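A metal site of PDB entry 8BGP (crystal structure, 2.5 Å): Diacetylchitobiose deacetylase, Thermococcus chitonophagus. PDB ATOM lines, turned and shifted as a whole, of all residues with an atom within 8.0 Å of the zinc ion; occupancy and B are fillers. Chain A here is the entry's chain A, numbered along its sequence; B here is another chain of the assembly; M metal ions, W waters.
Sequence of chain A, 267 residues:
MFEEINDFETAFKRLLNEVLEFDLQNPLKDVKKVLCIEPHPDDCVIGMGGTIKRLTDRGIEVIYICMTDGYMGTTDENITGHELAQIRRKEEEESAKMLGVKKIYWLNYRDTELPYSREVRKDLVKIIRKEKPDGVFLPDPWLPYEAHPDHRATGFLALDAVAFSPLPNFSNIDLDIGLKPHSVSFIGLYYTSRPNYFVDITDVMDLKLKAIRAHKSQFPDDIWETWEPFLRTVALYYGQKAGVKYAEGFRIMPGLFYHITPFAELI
A ring nitrogen (NE2) of His 40 sits at hydrogen-bond distance from the side-chain carboxylate (OD2) of Asp 150, 2.8 Å away. A ring nitrogen (ND1) of His 259 of chain B sits at hydrogen-bond distance from the side-chain carboxylate (OE2) of Glu 146 (2.8 Å). The side-chain carboxylate of Glu 38 sits at hydrogen-bond distance from the backbone NH of Asp 43 (3.4 Å). The side-chain carboxylate (OD1) of Asp 111 lies within hydrogen-bond range of a ring nitrogen (NE2) of His 40 (3.0 Å). The side-chain hydroxyl (OH) of Tyr 191 lies within hydrogen-bond range of the side-chain carboxylate (OD1) of Asp 43 (2.8 Å).
Water W1 lies within hydrogen-bond range of the side-chain carboxylate (OD1) of Asp 43 (2.7 Å), a ring nitrogen (NE2) of His 259 of chain B (3.3 Å) and the side-chain carboxylate (OD1) of Asp 42 (3.5 Å).
The zinc ion is bound by the side-chain carboxylate (OD2) of Asp 43, a ring nitrogen (ND1) of His 40, water W1 and a ring nitrogen (NE2) of His 151. The zinc ion has four donor atoms within binding distance. Slightly farther from the zinc ion lies the side-chain carboxylate (OD1) of Asp 43 (2.8 Å).
NE2 of His 259 of chain B touches the zinc ion (3.9 Å). Four residues have an atom within 4 Å of the zinc ion: His 40, Asp 43, His 151 and His 259 of chain B. The nearest printed residue that does not touch the zinc ion is Pro 39 (4.3 Å).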
ATOM      1  N   GLU A  38      -2.971  22.220 -11.351  1.00  0.00           N
ATOM      2  CA  GLU A  38      -3.431  21.021 -12.073  1.00  0.00           C
ATOM      3  C   GLU A  38      -4.842  20.706 -11.627  1.00  0.00           C
ATOM      4  O   GLU A  38      -5.154  20.722 -10.437  1.00  0.00           O
ATOM      5  CB  GLU A  38      -2.503  19.824 -11.840  1.00  0.00           C
ATOM      6  CG  GLU A  38      -2.205  19.475 -10.387  1.00  0.00           C
ATOM      7  CD  GLU A  38      -1.344  18.223 -10.184  1.00  0.00           C
ATOM      8  OE1 GLU A  38      -0.767  17.713 -11.194  1.00  0.00           O
ATOM      9  OE2 GLU A  38      -1.270  17.740  -9.029  1.00  0.00           O
ATOM     10  N   PRO A  39      -5.756  20.462 -12.590  1.00  0.00           N
ATOM     11  CA  PRO A  39      -7.109  20.011 -12.254  1.00  0.00           C
ATOM     12  C   PRO A  39      -7.144  18.653 -11.525  1.00  0.00           C
ATOM     13  O   PRO A  39      -7.889  18.502 -10.576  1.00  0.00           O
ATOM     14  CB  PRO A  39      -7.773  19.864 -13.631  1.00  0.00           C
ATOM     15  CG  PRO A  39      -6.950  20.749 -14.528  1.00  0.00           C
ATOM     16  CD  PRO A  39      -5.542  20.629 -14.028  1.00  0.00           C
ATOM     17  N   HIS A  40      -6.321  17.698 -11.990  1.00  0.00           N
ATOM     18  CA  HIS A  40      -6.248  16.327 -11.436  1.00  0.00           C
ATOM     19  C   HIS A  40      -4.816  15.980 -11.087  1.00  0.00           C
ATOM     20  O   HIS A  40      -3.904  16.529 -11.670  1.00  0.00           O
ATOM     21  CB  HIS A  40      -6.814  15.308 -12.427  1.00  0.00           C
ATOM     22  CG  HIS A  40      -8.185  15.624 -12.901  1.00  0.00           C
ATOM     23  ND1 HIS A  40      -8.409  16.114 -14.170  1.00  0.00           N
ATOM     24  CD2 HIS A  40      -9.393  15.521 -12.293  1.00  0.00           C
ATOM     25  CE1 HIS A  40      -9.698  16.296 -14.321  1.00  0.00           C
ATOM     26  NE2 HIS A  40     -10.338  15.935 -13.193  1.00  0.00           N
ATOM     27  N   PRO A  41      -4.601  15.044 -10.135  1.00  0.00           N
ATOM     28  CA  PRO A  41      -3.272  14.461  -9.931  1.00  0.00           C
ATOM     29  C   PRO A  41      -2.784  13.816 -11.237  1.00  0.00           C
ATOM     30  O   PRO A  41      -3.450  12.922 -11.705  1.00  0.00           O
ATOM     31  CB  PRO A  41      -3.489  13.421  -8.823  1.00  0.00           C
ATOM     32  CG  PRO A  41      -4.782  13.825  -8.155  1.00  0.00           C
ATOM     33  CD  PRO A  41      -5.602  14.505  -9.215  1.00  0.00           C
ATOM     34  N   ASP A  42      -1.685  14.330 -11.778  1.00  0.00           N
ATOM     35  CA  ASP A  42      -0.988  13.861 -13.012  1.00  0.00           C
ATOM     36  C   ASP A  42      -1.000  14.955 -14.082  1.00  0.00           C
ATOM     37  O   ASP A  42      -0.222  14.829 -15.041  1.00  0.00           O
ATOM     38  CB  ASP A  42      -1.482  12.501 -13.545  1.00  0.00           C
ATOM     39  CG  ASP A  42      -2.827  12.442 -14.279  1.00  0.00           C
ATOM     40  OD1 ASP A  42      -3.363  13.492 -14.708  1.00  0.00           O
ATOM     41  OD2 ASP A  42      -3.364  11.334 -14.437  1.00  0.00           O
ATOM     42  N   ASP A  43      -1.830  15.994 -13.958  1.00  0.00           N
ATOM     43  CA  ASP A  43      -2.049  16.947 -15.070  1.00  0.00           C
ATOM     44  C   ASP A  43      -0.771  17.785 -15.243  1.00  0.00           C
ATOM     45  O   ASP A  43      -0.384  18.056 -16.398  1.00  0.00           O
ATOM     46  CB  ASP A  43      -3.352  17.740 -14.914  1.00  0.00           C
ATOM     47  CG  ASP A  43      -4.568  17.047 -15.525  1.00  0.00           C
ATOM     48  OD1 ASP A  43      -4.409  16.406 -16.571  1.00  0.00           O
ATOM     49  OD2 ASP A  43      -5.678  17.138 -14.926  1.00  0.00           O
ATOM     50  N   CYS A  44      -0.106  18.146 -14.143  1.00  0.00           N
ATOM     51  CA  CYS A  44       1.138  18.968 -14.184  1.00  0.00           C
ATOM     52  C   CYS A  44       2.222  18.211 -14.946  1.00  0.00           C
ATOM     53  O   CYS A  44       2.857  18.808 -15.850  1.00  0.00           O
ATOM     54  CB  CYS A  44       1.632  19.302 -12.790  1.00  0.00           C
ATOM     55  SG  CYS A  44       0.946  20.867 -12.194  1.00  0.00           S
ATOM     56  N   ILE A  46       1.995  15.535 -16.978  1.00  0.00           N
ATOM     57  CA  ILE A  46       1.627  15.185 -18.394  1.00  0.00           C
ATOM     58  C   ILE A  46       1.735  16.452 -19.243  1.00  0.00           C
ATOM     59  O   ILE A  46       2.107  16.337 -20.430  1.00  0.00           O
ATOM     60  CB  ILE A  46       0.215  14.579 -18.516  1.00  0.00           C
ATOM     61  CG1 ILE A  46       0.089  13.234 -17.789  1.00  0.00           C
ATOM     62  CG2 ILE A  46      -0.177  14.461 -19.976  1.00  0.00           C
ATOM     63  CD1 ILE A  46      -1.339  12.757 -17.599  1.00  0.00           C
ATOM     64  N   THR A  68      -8.506  18.854  -7.477  1.00  0.00           N
ATOM     65  CA  THR A  68      -9.401  17.714  -7.165  1.00  0.00           C
ATOM     66  C   THR A  68      -8.608  16.558  -6.563  1.00  0.00           C
ATOM     67  O   THR A  68      -7.368  16.583  -6.595  1.00  0.00           O
ATOM     68  CB  THR A  68     -10.185  17.253  -8.396  1.00  0.00           C
ATOM     69  OG1 THR A  68      -9.279  16.667  -9.342  1.00  0.00           O
ATOM     70  CG2 THR A  68     -10.940  18.396  -9.066  1.00  0.00           C
ATOM     71  N   ARG A  88      -3.805   8.011  -5.324  1.00  0.00           N
ATOM     72  CA  ARG A  88      -3.332   9.032  -6.319  1.00  0.00           C
ATOM     73  C   ARG A  88      -2.556  10.136  -5.599  1.00  0.00           C
ATOM     74  O   ARG A  88      -1.759  10.795  -6.250  1.00  0.00           O
ATOM     75  CB  ARG A  88      -4.514   9.572  -7.121  1.00  0.00           C
ATOM     76  CG  ARG A  88      -5.119   8.526  -8.054  1.00  0.00           C
ATOM     77  CD  ARG A  88      -6.185   9.104  -8.947  1.00  0.00           C
ATOM     78  NE  ARG A  88      -5.613   9.974  -9.966  1.00  0.00           N
ATOM     79  CZ  ARG A  88      -6.305  10.529 -10.961  1.00  0.00           C
ATOM     80  NH1 ARG A  88      -7.603  10.307 -11.067  1.00  0.00           N
ATOM     81  NH2 ARG A  88      -5.683  11.290 -11.844  1.00  0.00           N
ATOM     82  N   ASP A 111     -13.274  15.117  -7.965  1.00  0.00           N
ATOM     83  CA  ASP A 111     -13.131  14.884  -9.426  1.00  0.00           C
ATOM     84  C   ASP A 111     -14.528  14.920 -10.030  1.00  0.00           C
ATOM     85  O   ASP A 111     -15.418  14.247  -9.479  1.00  0.00           O
ATOM     86  CB  ASP A 111     -12.399  13.558  -9.698  1.00  0.00           C
ATOM     87  CG  ASP A 111     -12.002  13.250 -11.141  1.00  0.00           C
ATOM     88  OD1 ASP A 111     -12.324  14.070 -12.043  1.00  0.00           O
ATOM     89  OD2 ASP A 111     -11.378  12.198 -11.349  1.00  0.00           O
ATOM     90  N   PRO A 139      -3.752  25.363 -17.035  1.00  0.00           N
ATOM     91  CA  PRO A 139      -4.208  24.846 -18.311  1.00  0.00           C
ATOM     92  C   PRO A 139      -5.021  25.915 -19.057  1.00  0.00           C
ATOM     93  O   PRO A 139      -5.784  26.593 -18.428  1.00  0.00           O
ATOM     94  CB  PRO A 139      -5.039  23.599 -17.958  1.00  0.00           C
ATOM     95  CG  PRO A 139      -5.489  23.847 -16.526  1.00  0.00           C
ATOM     96  CD  PRO A 139      -4.414  24.707 -15.886  1.00  0.00           C
ATOM     97  N   GLU A 146     -11.736  20.544 -25.577  1.00  0.00           N
ATOM     98  CA  GLU A 146     -11.591  20.132 -24.160  1.00  0.00           C
ATOM     99  C   GLU A 146     -12.974  19.909 -23.560  1.00  0.00           C
ATOM    100  O   GLU A 146     -13.682  20.878 -23.295  1.00  0.00           O
ATOM    101  CB  GLU A 146     -10.824  21.164 -23.324  1.00  0.00           C
ATOM    102  CG  GLU A 146     -10.566  20.698 -21.887  1.00  0.00           C
ATOM    103  CD  GLU A 146      -9.820  19.361 -21.760  1.00  0.00           C
ATOM    104  OE1 GLU A 146      -8.586  19.350 -22.058  1.00  0.00           O
ATOM    105  OE2 GLU A 146     -10.470  18.342 -21.362  1.00  0.00           O
ATOM    106  N   HIS A 148     -13.517  18.108 -20.617  1.00  0.00           N
ATOM    107  CA  HIS A 148     -13.489  17.892 -19.144  1.00  0.00           C
ATOM    108  C   HIS A 148     -13.850  19.179 -18.431  1.00  0.00           C
ATOM    109  O   HIS A 148     -13.135  20.161 -18.512  1.00  0.00           O
ATOM    110  CB  HIS A 148     -12.169  17.284 -18.657  1.00  0.00           C
ATOM    111  CG  HIS A 148     -12.370  16.447 -17.427  1.00  0.00           C
ATOM    112  ND1 HIS A 148     -12.966  16.952 -16.273  1.00  0.00           N
ATOM    113  CD2 HIS A 148     -12.141  15.138 -17.188  1.00  0.00           C
ATOM    114  CE1 HIS A 148     -13.052  16.013 -15.365  1.00  0.00           C
ATOM    115  NE2 HIS A 148     -12.538  14.901 -15.900  1.00  0.00           N
ATOM    116  N   ASP A 150     -13.612  19.956 -15.281  1.00  0.00           N
ATOM    117  CA  ASP A 150     -12.566  20.305 -14.301  1.00  0.00           C
ATOM    118  C   ASP A 150     -11.434  21.095 -14.992  1.00  0.00           C
ATOM    119  O   ASP A 150     -10.884  22.033 -14.382  1.00  0.00           O
ATOM    120  CB  ASP A 150     -12.036  19.071 -13.567  1.00  0.00           C
ATOM    121  CG  ASP A 150     -13.055  18.335 -12.704  1.00  0.00           C
ATOM    122  OD1 ASP A 150     -14.129  18.910 -12.420  1.00  0.00           O
ATOM    123  OD2 ASP A 150     -12.755  17.151 -12.335  1.00  0.00           O
ATOM    124  N   HIS A 151     -11.094  20.755 -16.234  1.00  0.00           N
ATOM    125  CA  HIS A 151     -10.034  21.459 -17.004  1.00  0.00           C
ATOM    126  C   HIS A 151     -10.489  22.873 -17.358  1.00  0.00           C
ATOM    127  O   HIS A 151      -9.730  23.823 -17.108  1.00  0.00           O
ATOM    128  CB  HIS A 151      -9.625  20.664 -18.249  1.00  0.00           C
ATOM    129  CG  HIS A 151      -8.651  19.566 -17.923  1.00  0.00           C
ATOM    130  ND1 HIS A 151      -7.457  19.429 -18.621  1.00  0.00           N
ATOM    131  CD2 HIS A 151      -8.668  18.628 -16.946  1.00  0.00           C
ATOM    132  CE1 HIS A 151      -6.818  18.389 -18.135  1.00  0.00           C
ATOM    133  NE2 HIS A 151      -7.547  17.885 -17.089  1.00  0.00           N
ATOM    134  N   THR A 154     -10.720  24.972 -14.035  1.00  0.00           N
ATOM    135  CA  THR A 154      -9.379  25.227 -13.448  1.00  0.00           C
ATOM    136  C   THR A 154      -8.703  26.407 -14.149  1.00  0.00           C
ATOM    137  O   THR A 154      -8.185  27.274 -13.451  1.00  0.00           O
ATOM    138  CB  THR A 154      -8.494  23.993 -13.501  1.00  0.00           C
ATOM    139  OG1 THR A 154      -9.132  22.970 -12.733  1.00  0.00           O
ATOM    140  CG2 THR A 154      -7.106  24.250 -12.958  1.00  0.00           C
ATOM    141  N   TYR A 190      -0.289  26.008 -20.172  1.00  0.00           N
ATOM    142  CA  TYR A 190       0.109  24.703 -20.758  1.00  0.00           C
ATOM    143  C   TYR A 190      -1.138  24.001 -21.297  1.00  0.00           C
ATOM    144  O   TYR A 190      -2.258  24.563 -21.158  1.00  0.00           O
ATOM    145  CB  TYR A 190       0.868  23.829 -19.754  1.00  0.00           C
ATOM    146  CG  TYR A 190       0.116  23.338 -18.547  1.00  0.00           C
ATOM    147  CD1 TYR A 190       0.010  24.084 -17.406  1.00  0.00           C
ATOM    148  CD2 TYR A 190      -0.412  22.065 -18.509  1.00  0.00           C
ATOM    149  CE1 TYR A 190      -0.627  23.613 -16.274  1.00  0.00           C
ATOM    150  CE2 TYR A 190      -1.072  21.579 -17.401  1.00  0.00           C
ATOM    151  CZ  TYR A 190      -1.164  22.341 -16.267  1.00  0.00           C
ATOM    152  OH  TYR A 190      -1.794  21.866 -15.147  1.00  0.00           O
ATOM    153  N   TYR A 191      -0.958  22.839 -21.916  1.00  0.00           N
ATOM    154  CA  TYR A 191      -2.033  22.096 -22.620  1.00  0.00           C
ATOM    155  C   TYR A 191      -2.709  23.066 -23.586  1.00  0.00           C
ATOM    156  O   TYR A 191      -3.969  23.227 -23.538  1.00  0.00           O
ATOM    157  CB  TYR A 191      -3.100  21.606 -21.652  1.00  0.00           C
ATOM    158  CG  TYR A 191      -2.842  20.362 -20.851  1.00  0.00           C
ATOM    159  CD1 TYR A 191      -2.125  19.273 -21.343  1.00  0.00           C
ATOM    160  CD2 TYR A 191      -3.430  20.238 -19.596  1.00  0.00           C
ATOM    161  CE1 TYR A 191      -1.966  18.132 -20.583  1.00  0.00           C
ATOM    162  CE2 TYR A 191      -3.262  19.101 -18.825  1.00  0.00           C
ATOM    163  CZ  TYR A 191      -2.531  18.041 -19.320  1.00  0.00           C
ATOM    164  OH  TYR A 191      -2.430  16.956 -18.512  1.00  0.00           O
ATOM    165  N   HIS B 259      -9.878  15.364 -24.894  1.00  0.00           N
ATOM    166  CA  HIS B 259      -9.072  15.607 -23.667  1.00  0.00           C
ATOM    167  C   HIS B 259      -7.622  15.948 -24.078  1.00  0.00           C
ATOM    168  O   HIS B 259      -7.040  15.154 -24.797  1.00  0.00           O
ATOM    169  CB  HIS B 259      -9.218  14.437 -22.699  1.00  0.00           C
ATOM    170  CG  HIS B 259      -8.844  14.782 -21.295  1.00  0.00           C
ATOM    171  ND1 HIS B 259      -9.440  15.835 -20.594  1.00  0.00           N
ATOM    172  CD2 HIS B 259      -7.908  14.238 -20.458  1.00  0.00           C
ATOM    173  CE1 HIS B 259      -8.912  15.892 -19.385  1.00  0.00           C
ATOM    174  NE2 HIS B 259      -7.942  14.927 -19.273  1.00  0.00           N
ATOM    175  N   ILE B 260      -7.159  17.143 -23.697  1.00  0.00           N
ATOM    176  CA  ILE B 260      -5.745  17.631 -23.687  1.00  0.00           C
ATOM    177  C   ILE B 260      -4.997  17.331 -24.996  1.00  0.00           C
ATOM    178  O   ILE B 260      -3.781  17.113 -24.952  1.00  0.00           O
ATOM    179  CB  ILE B 260      -5.009  17.063 -22.471  1.00  0.00           C
ATOM    180  CG1 ILE B 260      -4.877  15.535 -22.507  1.00  0.00           C
ATOM    181  CG2 ILE B 260      -5.675  17.565 -21.199  1.00  0.00           C
ATOM    182  CD1 ILE B 260      -3.828  14.998 -21.572  1.00  0.00           C
HETATM  183 ZN    ZN M   1      -7.072  16.178 -15.632  1.00  0.00          ZN
HETATM  184  O   HOH W   1      -6.228  14.379 -16.493  1.00  0.00           O
